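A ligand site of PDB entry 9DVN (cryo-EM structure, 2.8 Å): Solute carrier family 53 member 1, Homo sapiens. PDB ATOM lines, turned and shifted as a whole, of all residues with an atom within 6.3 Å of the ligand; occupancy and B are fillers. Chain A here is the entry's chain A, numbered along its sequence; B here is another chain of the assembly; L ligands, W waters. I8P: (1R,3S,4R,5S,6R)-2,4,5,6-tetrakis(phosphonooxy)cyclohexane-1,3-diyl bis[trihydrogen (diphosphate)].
The side-chain amino group (NZ) of Lys 165 lies within salt-bridge range of an oxygen (O22) of the ligand (2.6 Å).
The backbone NH (N) of Lys 2 lies within hydrogen-bond range of an oxygen (O31) of the ligand, 2.6 Å away.
The side-chain hydroxyl (OH) of Tyr 22 sits close to an oxygen (O51) of the ligand, 3.4 Å away.
The backbone NH (N) of Phe 3 lies within hydrogen-bond range of an oxygen (O51) of the ligand.
The side-chain amino group (NZ) of Lys 162 is in salt-bridge range of an oxygen (O61) of the ligand, 3.3 Å away.
NZ of Lys 26 lies within salt-bridge range of O61 of the ligand, 2.6 Å away.
The backbone NH of Ala 4 sits at hydrogen-bond distance from an oxygen (O71) of the ligand (3.0 Å).
An oxygen (O23) of the ligand is in salt-bridge range of the guanidinium group (NH2) of Arg 219 of chain B, 2.6 Å away.
The side-chain amide nitrogen (NE2) of Gln 212 of chain B lies within hydrogen-bond range of an oxygen (O32) of the ligand, at 3.3 Å.
An oxygen (O65) of the ligand is in salt-bridge range of the side-chain amino group (NZ) of Lys 158 (2.5 Å).
SD of Met 1 sits close to O35 of the ligand, at 3.0 Å.
The guanidinium group (NH1) of Arg 211 of chain B lies within salt-bridge range of an oxygen (O34) of the ligand.
The side-chain amino group (NZ) of Lys 161 is in salt-bridge range of an oxygen (O75) of the ligand, 2.5 Å away.
The side-chain sulfur (SD) of Met 1 lies within hydrogen-bond range of the guanidinium group (NH1) of Arg 219 of chain B, 3.5 Å away.
The side-chain hydroxyl (OH) of Tyr 30 is in hydrogen-bond range of the side-chain amino group (NZ) of Lys 26 (2.5 Å).
Merely in contact with the ligand: Met 215 of chain B (3.6 Å).
14 residues have an atom within 4 Å of the ligand: Met 1, Lys 2, Phe 3, Ala 4, Tyr 22, Lys 26, Lys 158, Lys 161, Lys 162, Lys 165, Arg 211 of chain B, Gln 212 of chain B, Met 215 of chain B and Arg 219 of chain B.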
ATOM      1  N   MET A   1     -14.304  23.421 -16.210  1.00  0.00           N
ATOM      2  CA  MET A   1     -15.538  23.213 -15.382  1.00  0.00           C
ATOM      3  C   MET A   1     -16.768  23.143 -16.268  1.00  0.00           C
ATOM      4  O   MET A   1     -16.992  24.000 -17.118  1.00  0.00           O
ATOM      5  CB  MET A   1     -15.691  24.351 -14.361  1.00  0.00           C
ATOM      6  CG  MET A   1     -14.630  24.360 -13.278  1.00  0.00           C
ATOM      7  SD  MET A   1     -14.499  22.800 -12.367  1.00  0.00           S
ATOM      8  CE  MET A   1     -16.221  22.450 -12.026  1.00  0.00           C
ATOM      9  N   LYS A   2     -17.579  22.104 -16.058  1.00  0.00           N
ATOM     10  CA  LYS A   2     -18.794  21.880 -16.833  1.00  0.00           C
ATOM     11  C   LYS A   2     -18.489  21.898 -18.330  1.00  0.00           C
ATOM     12  O   LYS A   2     -18.991  22.716 -19.097  1.00  0.00           O
ATOM     13  CB  LYS A   2     -19.873  22.911 -16.479  1.00  0.00           C
ATOM     14  CG  LYS A   2     -20.432  22.817 -15.059  1.00  0.00           C
ATOM     15  CD  LYS A   2     -21.472  23.897 -14.790  1.00  0.00           C
ATOM     16  CE  LYS A   2     -22.043  23.770 -13.382  1.00  0.00           C
ATOM     17  NZ  LYS A   2     -23.045  24.842 -13.094  1.00  0.00           N
ATOM     18  N   PHE A   3     -17.624  20.958 -18.726  1.00  0.00           N
ATOM     19  CA  PHE A   3     -17.160  20.915 -20.105  1.00  0.00           C
ATOM     20  C   PHE A   3     -18.260  20.535 -21.097  1.00  0.00           C
ATOM     21  O   PHE A   3     -18.071  20.746 -22.303  1.00  0.00           O
ATOM     22  CB  PHE A   3     -15.996  19.929 -20.245  1.00  0.00           C
ATOM     23  CG  PHE A   3     -15.416  19.854 -21.617  1.00  0.00           C
ATOM     24  CD1 PHE A   3     -14.568  20.850 -22.086  1.00  0.00           C
ATOM     25  CD2 PHE A   3     -15.733  18.808 -22.460  1.00  0.00           C
ATOM     26  CE1 PHE A   3     -14.038  20.780 -23.359  1.00  0.00           C
ATOM     27  CE2 PHE A   3     -15.207  18.734 -23.740  1.00  0.00           C
ATOM     28  CZ  PHE A   3     -14.354  19.725 -24.182  1.00  0.00           C
ATOM     29  N   ALA A   4     -19.386  20.004 -20.637  1.00  0.00           N
ATOM     30  CA  ALA A   4     -20.455  19.614 -21.549  1.00  0.00           C
ATOM     31  C   ALA A   4     -21.000  20.828 -22.298  1.00  0.00           C
ATOM     32  O   ALA A   4     -21.071  20.829 -23.535  1.00  0.00           O
ATOM     33  CB  ALA A   4     -21.572  18.900 -20.792  1.00  0.00           C
ATOM     34  N   GLU A   5     -21.393  21.867 -21.568  1.00  0.00           N
ATOM     35  CA  GLU A   5     -21.930  23.058 -22.213  1.00  0.00           C
ATOM     36  C   GLU A   5     -20.851  23.792 -23.011  1.00  0.00           C
ATOM     37  O   GLU A   5     -21.144  24.365 -24.061  1.00  0.00           O
ATOM     38  CB  GLU A   5     -22.571  23.995 -21.192  1.00  0.00           C
ATOM     39  CG  GLU A   5     -21.710  24.281 -19.975  1.00  0.00           C
ATOM     40  CD  GLU A   5     -22.274  23.664 -18.708  1.00  0.00           C
ATOM     41  OE1 GLU A   5     -22.826  22.542 -18.779  1.00  0.00           O
ATOM     42  OE2 GLU A   5     -22.167  24.302 -17.630  1.00  0.00           O
ATOM     43  N   TYR A  22     -19.189  13.776 -25.801  1.00  0.00           N
ATOM     44  CA  TYR A  22     -18.907  13.858 -24.367  1.00  0.00           C
ATOM     45  C   TYR A  22     -20.117  13.433 -23.545  1.00  0.00           C
ATOM     46  O   TYR A  22     -19.978  12.687 -22.567  1.00  0.00           O
ATOM     47  CB  TYR A  22     -18.480  15.280 -24.010  1.00  0.00           C
ATOM     48  CG  TYR A  22     -17.691  15.396 -22.734  1.00  0.00           C
ATOM     49  CD1 TYR A  22     -16.354  15.048 -22.677  1.00  0.00           C
ATOM     50  CD2 TYR A  22     -18.289  15.871 -21.569  1.00  0.00           C
ATOM     51  CE1 TYR A  22     -15.628  15.155 -21.501  1.00  0.00           C
ATOM     52  CE2 TYR A  22     -17.571  15.983 -20.390  1.00  0.00           C
ATOM     53  CZ  TYR A  22     -16.238  15.624 -20.364  1.00  0.00           C
ATOM     54  OH  TYR A  22     -15.523  15.739 -19.199  1.00  0.00           O
ATOM     55  N   GLU A  23     -21.308  13.892 -23.923  1.00  0.00           N
ATOM     56  CA  GLU A  23     -22.509  13.528 -23.185  1.00  0.00           C
ATOM     57  C   GLU A  23     -22.783  12.036 -23.278  1.00  0.00           C
ATOM     58  O   GLU A  23     -23.224  11.417 -22.301  1.00  0.00           O
ATOM     59  CB  GLU A  23     -23.706  14.331 -23.703  1.00  0.00           C
ATOM     60  CG  GLU A  23     -23.820  15.727 -23.129  1.00  0.00           C
ATOM     61  CD  GLU A  23     -24.463  15.741 -21.758  1.00  0.00           C
ATOM     62  OE1 GLU A  23     -24.481  14.685 -21.094  1.00  0.00           O
ATOM     63  OE2 GLU A  23     -24.947  16.815 -21.341  1.00  0.00           O
ATOM     64  N   LYS A  26     -20.477  10.382 -20.838  1.00  0.00           N
ATOM     65  CA  LYS A  26     -20.955  10.613 -19.483  1.00  0.00           C
ATOM     66  C   LYS A  26     -22.125   9.683 -19.158  1.00  0.00           C
ATOM     67  O   LYS A  26     -22.182   9.095 -18.072  1.00  0.00           O
ATOM     68  CB  LYS A  26     -21.371  12.067 -19.309  1.00  0.00           C
ATOM     69  CG  LYS A  26     -20.225  13.063 -19.343  1.00  0.00           C
ATOM     70  CD  LYS A  26     -20.731  14.501 -19.382  1.00  0.00           C
ATOM     71  CE  LYS A  26     -21.566  14.853 -18.153  1.00  0.00           C
ATOM     72  NZ  LYS A  26     -20.861  14.536 -16.878  1.00  0.00           N
ATOM     73  N   TYR A  30     -22.167   6.823 -16.244  1.00  0.00           N
ATOM     74  CA  TYR A  30     -23.161   6.878 -15.172  1.00  0.00           C
ATOM     75  C   TYR A  30     -24.046   5.635 -15.181  1.00  0.00           C
ATOM     76  O   TYR A  30     -24.373   5.095 -14.114  1.00  0.00           O
ATOM     77  CB  TYR A  30     -24.013   8.143 -15.313  1.00  0.00           C
ATOM     78  CG  TYR A  30     -23.216   9.434 -15.217  1.00  0.00           C
ATOM     79  CD1 TYR A  30     -21.963   9.455 -14.618  1.00  0.00           C
ATOM     80  CD2 TYR A  30     -23.720  10.626 -15.721  1.00  0.00           C
ATOM     81  CE1 TYR A  30     -21.237  10.632 -14.525  1.00  0.00           C
ATOM     82  CE2 TYR A  30     -22.999  11.798 -15.636  1.00  0.00           C
ATOM     83  CZ  TYR A  30     -21.761  11.795 -15.038  1.00  0.00           C
ATOM     84  OH  TYR A  30     -21.040  12.968 -14.953  1.00  0.00           O
ATOM     85  N   ARG A 157      -9.333  14.276 -23.277  1.00  0.00           N
ATOM     86  CA  ARG A 157      -8.639  14.318 -21.999  1.00  0.00           C
ATOM     87  C   ARG A 157      -9.637  14.402 -20.845  1.00  0.00           C
ATOM     88  O   ARG A 157      -9.509  13.670 -19.855  1.00  0.00           O
ATOM     89  CB  ARG A 157      -7.682  15.504 -21.963  1.00  0.00           C
ATOM     90  CG  ARG A 157      -6.742  15.514 -20.768  1.00  0.00           C
ATOM     91  CD  ARG A 157      -5.881  16.761 -20.731  1.00  0.00           C
ATOM     92  NE  ARG A 157      -6.681  17.979 -20.620  1.00  0.00           N
ATOM     93  CZ  ARG A 157      -7.333  18.360 -19.523  1.00  0.00           C
ATOM     94  NH1 ARG A 157      -7.305  17.624 -18.419  1.00  0.00           N
ATOM     95  NH2 ARG A 157      -8.032  19.491 -19.538  1.00  0.00           N
ATOM     96  N   LYS A 158     -10.646  15.261 -20.968  1.00  0.00           N
ATOM     97  CA  LYS A 158     -11.615  15.434 -19.890  1.00  0.00           C
ATOM     98  C   LYS A 158     -12.408  14.154 -19.653  1.00  0.00           C
ATOM     99  O   LYS A 158     -12.622  13.753 -18.504  1.00  0.00           O
ATOM    100  CB  LYS A 158     -12.555  16.596 -20.220  1.00  0.00           C
ATOM    101  CG  LYS A 158     -11.862  17.940 -20.357  1.00  0.00           C
ATOM    102  CD  LYS A 158     -11.853  18.713 -19.048  1.00  0.00           C
ATOM    103  CE  LYS A 158     -11.492  20.177 -19.273  1.00  0.00           C
ATOM    104  NZ  LYS A 158     -11.714  20.996 -18.049  1.00  0.00           N
ATOM    105  N   LYS A 161     -10.226  11.529 -18.019  1.00  0.00           N
ATOM    106  CA  LYS A 161     -10.029  11.862 -16.612  1.00  0.00           C
ATOM    107  C   LYS A 161     -11.272  11.526 -15.794  1.00  0.00           C
ATOM    108  O   LYS A 161     -11.170  10.969 -14.688  1.00  0.00           O
ATOM    109  CB  LYS A 161      -9.675  13.340 -16.472  1.00  0.00           C
ATOM    110  CG  LYS A 161      -9.502  13.821 -15.043  1.00  0.00           C
ATOM    111  CD  LYS A 161      -9.322  15.333 -14.979  1.00  0.00           C
ATOM    112  CE  LYS A 161     -10.611  16.071 -15.323  1.00  0.00           C
ATOM    113  NZ  LYS A 161     -10.541  17.522 -14.994  1.00  0.00           N
ATOM    114  N   LYS A 162     -12.454  11.840 -16.322  1.00  0.00           N
ATOM    115  CA  LYS A 162     -13.688  11.517 -15.613  1.00  0.00           C
ATOM    116  C   LYS A 162     -13.861  10.023 -15.461  1.00  0.00           C
ATOM    117  O   LYS A 162     -14.284   9.529 -14.409  1.00  0.00           O
ATOM    118  CB  LYS A 162     -14.884  12.136 -16.346  1.00  0.00           C
ATOM    119  CG  LYS A 162     -16.234  11.842 -15.712  1.00  0.00           C
ATOM    120  CD  LYS A 162     -17.390  12.337 -16.575  1.00  0.00           C
ATOM    121  CE  LYS A 162     -17.348  13.844 -16.780  1.00  0.00           C
ATOM    122  NZ  LYS A 162     -17.349  14.591 -15.489  1.00  0.00           N
ATOM    123  N   LYS A 165     -11.558   8.851 -12.743  1.00  0.00           N
ATOM    124  CA  LYS A 165     -12.069   9.208 -11.428  1.00  0.00           C
ATOM    125  C   LYS A 165     -13.211   8.294 -11.009  1.00  0.00           C
ATOM    126  O   LYS A 165     -13.262   7.824  -9.863  1.00  0.00           O
ATOM    127  CB  LYS A 165     -12.534  10.676 -11.432  1.00  0.00           C
ATOM    128  CG  LYS A 165     -12.924  11.202 -10.061  1.00  0.00           C
ATOM    129  CD  LYS A 165     -13.524  12.587 -10.138  1.00  0.00           C
ATOM    130  CE  LYS A 165     -14.889  12.576 -10.802  1.00  0.00           C
ATOM    131  NZ  LYS A 165     -15.664  13.816 -10.544  1.00  0.00           N
ATOM    132  N   ILE A 166     -14.145   8.029 -11.928  1.00  0.00           N
ATOM    133  CA  ILE A 166     -15.311   7.230 -11.576  1.00  0.00           C
ATOM    134  C   ILE A 166     -14.921   5.779 -11.311  1.00  0.00           C
ATOM    135  O   ILE A 166     -15.356   5.164 -10.326  1.00  0.00           O
ATOM    136  CB  ILE A 166     -16.376   7.326 -12.680  1.00  0.00           C
ATOM    137  CG1 ILE A 166     -16.937   8.753 -12.756  1.00  0.00           C
ATOM    138  CG2 ILE A 166     -17.505   6.327 -12.437  1.00  0.00           C
ATOM    139  CD1 ILE A 166     -17.714   9.048 -14.021  1.00  0.00           C
ATOM    140  N   ARG B 211     -15.166  14.214  -1.825  1.00  0.00           N
ATOM    141  CA  ARG B 211     -14.313  15.130  -2.577  1.00  0.00           C
ATOM    142  C   ARG B 211     -15.133  16.226  -3.238  1.00  0.00           C
ATOM    143  O   ARG B 211     -14.699  17.385  -3.298  1.00  0.00           O
ATOM    144  CB  ARG B 211     -13.496  14.369  -3.610  1.00  0.00           C
ATOM    145  CG  ARG B 211     -12.309  15.162  -4.151  1.00  0.00           C
ATOM    146  CD  ARG B 211     -11.467  14.344  -5.112  1.00  0.00           C
ATOM    147  NE  ARG B 211     -10.235  15.035  -5.471  1.00  0.00           N
ATOM    148  CZ  ARG B 211     -10.177  16.124  -6.223  1.00  0.00           C
ATOM    149  NH1 ARG B 211     -11.266  16.680  -6.733  1.00  0.00           N
ATOM    150  NH2 ARG B 211      -8.987  16.672  -6.478  1.00  0.00           N
ATOM    151  N   GLN B 212     -16.314  15.883  -3.758  1.00  0.00           N
ATOM    152  CA  GLN B 212     -17.144  16.885  -4.422  1.00  0.00           C
ATOM    153  C   GLN B 212     -17.558  17.983  -3.455  1.00  0.00           C
ATOM    154  O   GLN B 212     -17.523  19.178  -3.805  1.00  0.00           O
ATOM    155  CB  GLN B 212     -18.372  16.218  -5.038  1.00  0.00           C
ATOM    156  CG  GLN B 212     -19.261  17.159  -5.844  1.00  0.00           C
ATOM    157  CD  GLN B 212     -20.486  16.469  -6.406  1.00  0.00           C
ATOM    158  OE1 GLN B 212     -21.610  16.879  -6.145  1.00  0.00           O
ATOM    159  NE2 GLN B 212     -20.265  15.410  -7.180  1.00  0.00           N
ATOM    160  N   MET B 215     -14.576  20.238  -2.830  1.00  0.00           N
ATOM    161  CA  MET B 215     -14.224  21.064  -3.982  1.00  0.00           C
ATOM    162  C   MET B 215     -15.267  22.141  -4.244  1.00  0.00           C
ATOM    163  O   MET B 215     -14.944  23.188  -4.814  1.00  0.00           O
ATOM    164  CB  MET B 215     -14.059  20.181  -5.223  1.00  0.00           C
ATOM    165  CG  MET B 215     -12.759  20.393  -6.005  1.00  0.00           C
ATOM    166  SD  MET B 215     -11.275  20.491  -4.985  1.00  0.00           S
ATOM    167  CE  MET B 215     -11.487  19.061  -3.914  1.00  0.00           C
ATOM    168  N   LYS B 216     -16.525  21.902  -3.844  1.00  0.00           N
ATOM    169  CA  LYS B 216     -17.553  22.921  -4.025  1.00  0.00           C
ATOM    170  C   LYS B 216     -17.200  24.196  -3.280  1.00  0.00           C
ATOM    171  O   LYS B 216     -17.600  25.297  -3.705  1.00  0.00           O
ATOM    172  CB  LYS B 216     -18.903  22.388  -3.544  1.00  0.00           C
ATOM    173  CG  LYS B 216     -20.100  23.137  -4.110  1.00  0.00           C
ATOM    174  CD  LYS B 216     -21.406  22.549  -3.612  1.00  0.00           C
ATOM    175  CE  LYS B 216     -21.844  23.188  -2.303  1.00  0.00           C
ATOM    176  NZ  LYS B 216     -22.429  22.192  -1.363  1.00  0.00           N
ATOM    177  N   ARG B 219     -12.920  25.328  -4.637  1.00  0.00           N
ATOM    178  CA  ARG B 219     -12.728  25.878  -5.986  1.00  0.00           C
ATOM    179  C   ARG B 219     -12.858  27.398  -5.956  1.00  0.00           C
ATOM    180  O   ARG B 219     -13.699  27.961  -5.262  1.00  0.00           O
ATOM    181  CB  ARG B 219     -13.746  25.284  -6.958  1.00  0.00           C
ATOM    182  CG  ARG B 219     -13.226  25.175  -8.377  1.00  0.00           C
ATOM    183  CD  ARG B 219     -14.258  24.561  -9.313  1.00  0.00           C
ATOM    184  NE  ARG B 219     -14.795  23.311  -8.796  1.00  0.00           N
ATOM    185  CZ  ARG B 219     -14.174  22.143  -8.840  1.00  0.00           C
ATOM    186  NH1 ARG B 219     -12.967  22.031  -9.370  1.00  0.00           N
ATOM    187  NH2 ARG B 219     -14.768  21.065  -8.334  1.00  0.00           N
HETATM  188  C1  I8P L   1     -15.494  17.550 -13.702  1.00  0.00           C
HETATM  189  C2  I8P L   1     -15.830  16.905 -12.316  1.00  0.00           C
HETATM  190  C3  I8P L   1     -14.808  17.355 -11.176  1.00  0.00           C
HETATM  191  C4  I8P L   1     -13.373  17.763 -11.722  1.00  0.00           C
HETATM  192  C5  I8P L   1     -13.509  18.787 -12.914  1.00  0.00           C
HETATM  193  C6  I8P L   1     -14.927  18.979 -13.488  1.00  0.00           C
HETATM  194  O11 I8P L   1     -16.650  17.568 -14.489  1.00  0.00           O
HETATM  195  O12 I8P L   1     -17.126  17.145 -11.926  1.00  0.00           O
HETATM  196  O13 I8P L   1     -15.391  18.384 -10.486  1.00  0.00           O
HETATM  197  O14 I8P L   1     -12.739  16.633 -12.209  1.00  0.00           O
HETATM  198  O15 I8P L   1     -13.109  20.018 -12.394  1.00  0.00           O
HETATM  199  O16 I8P L   1     -14.762  19.652 -14.703  1.00  0.00           O
HETATM  200  O21 I8P L   1     -18.838  18.571 -13.300  1.00  0.00           O
HETATM  201  O22 I8P L   1     -17.808  14.602 -11.741  1.00  0.00           O
HETATM  202  O23 I8P L   1     -16.657  19.281  -8.278  1.00  0.00           O
HETATM  203  O24 I8P L   1     -10.197  16.875 -11.240  1.00  0.00           O
HETATM  204  O25 I8P L   1     -10.670  20.023 -11.329  1.00  0.00           O
HETATM  205  O26 I8P L   1     -13.002  18.143 -16.032  1.00  0.00           O
HETATM  206  O31 I8P L   1     -17.350  20.090 -14.431  1.00  0.00           O
HETATM  207  O32 I8P L   1     -18.756  16.184 -10.068  1.00  0.00           O
HETATM  208  O33 I8P L   1     -14.552  18.042  -8.073  1.00  0.00           O
HETATM  209  O34 I8P L   1     -11.776  15.329 -10.112  1.00  0.00           O
HETATM  210  O35 I8P L   1     -11.593  22.097 -12.617  1.00  0.00           O
HETATM  211  O36 I8P L   1     -14.253  20.027 -17.260  1.00  0.00           O
HETATM  212  O41 I8P L   1     -18.710  18.495 -15.805  1.00  0.00           O
HETATM  213  O42 I8P L   1     -19.609  16.130 -12.378  1.00  0.00           O
HETATM  214  O43 I8P L   1     -16.583  16.771  -8.712  1.00  0.00           O
HETATM  215  O44 I8P L   1     -10.808  14.903 -12.442  1.00  0.00           O
HETATM  216  O45 I8P L   1     -11.001  20.154 -13.804  1.00  0.00           O
HETATM  217  O46 I8P L   1     -15.359  17.924 -16.585  1.00  0.00           O
HETATM  218  O51 I8P L   1     -17.606  18.146 -18.087  1.00  0.00           O
HETATM  219  O55 I8P L   1      -8.845  21.683 -14.055  1.00  0.00           O
HETATM  220  O61 I8P L   1     -19.225  16.478 -17.375  1.00  0.00           O
HETATM  221  O65 I8P L   1     -10.372  21.380 -15.985  1.00  0.00           O
HETATM  222  O71 I8P L   1     -20.067  18.701 -18.058  1.00  0.00           O
HETATM  223  O75 I8P L   1      -9.083  19.489 -15.340  1.00  0.00           O
HETATM  224  PA1 I8P L   1     -17.870  18.647 -14.436  1.00  0.00           P
HETATM  225  PA2 I8P L   1     -18.345  16.017 -11.566  1.00  0.00           P
HETATM  226  PA3 I8P L   1     -15.853  18.160  -8.861  1.00  0.00           P
HETATM  227  PA4 I8P L   1     -11.378  15.954 -11.418  1.00  0.00           P
HETATM  228  PA5 I8P L   1     -11.605  20.587 -12.389  1.00  0.00           P
HETATM  229  PA6 I8P L   1     -14.283  18.961 -16.199  1.00  0.00           P
HETATM  230  PB1 I8P L   1     -18.929  17.984 -17.320  1.00  0.00           P
HETATM  231  PB5 I8P L   1      -9.821  20.706 -14.697  1.00  0.00           P
HETATM  232  O   HOH W   1      -8.369  18.419 -12.159  1.00  0.00           O
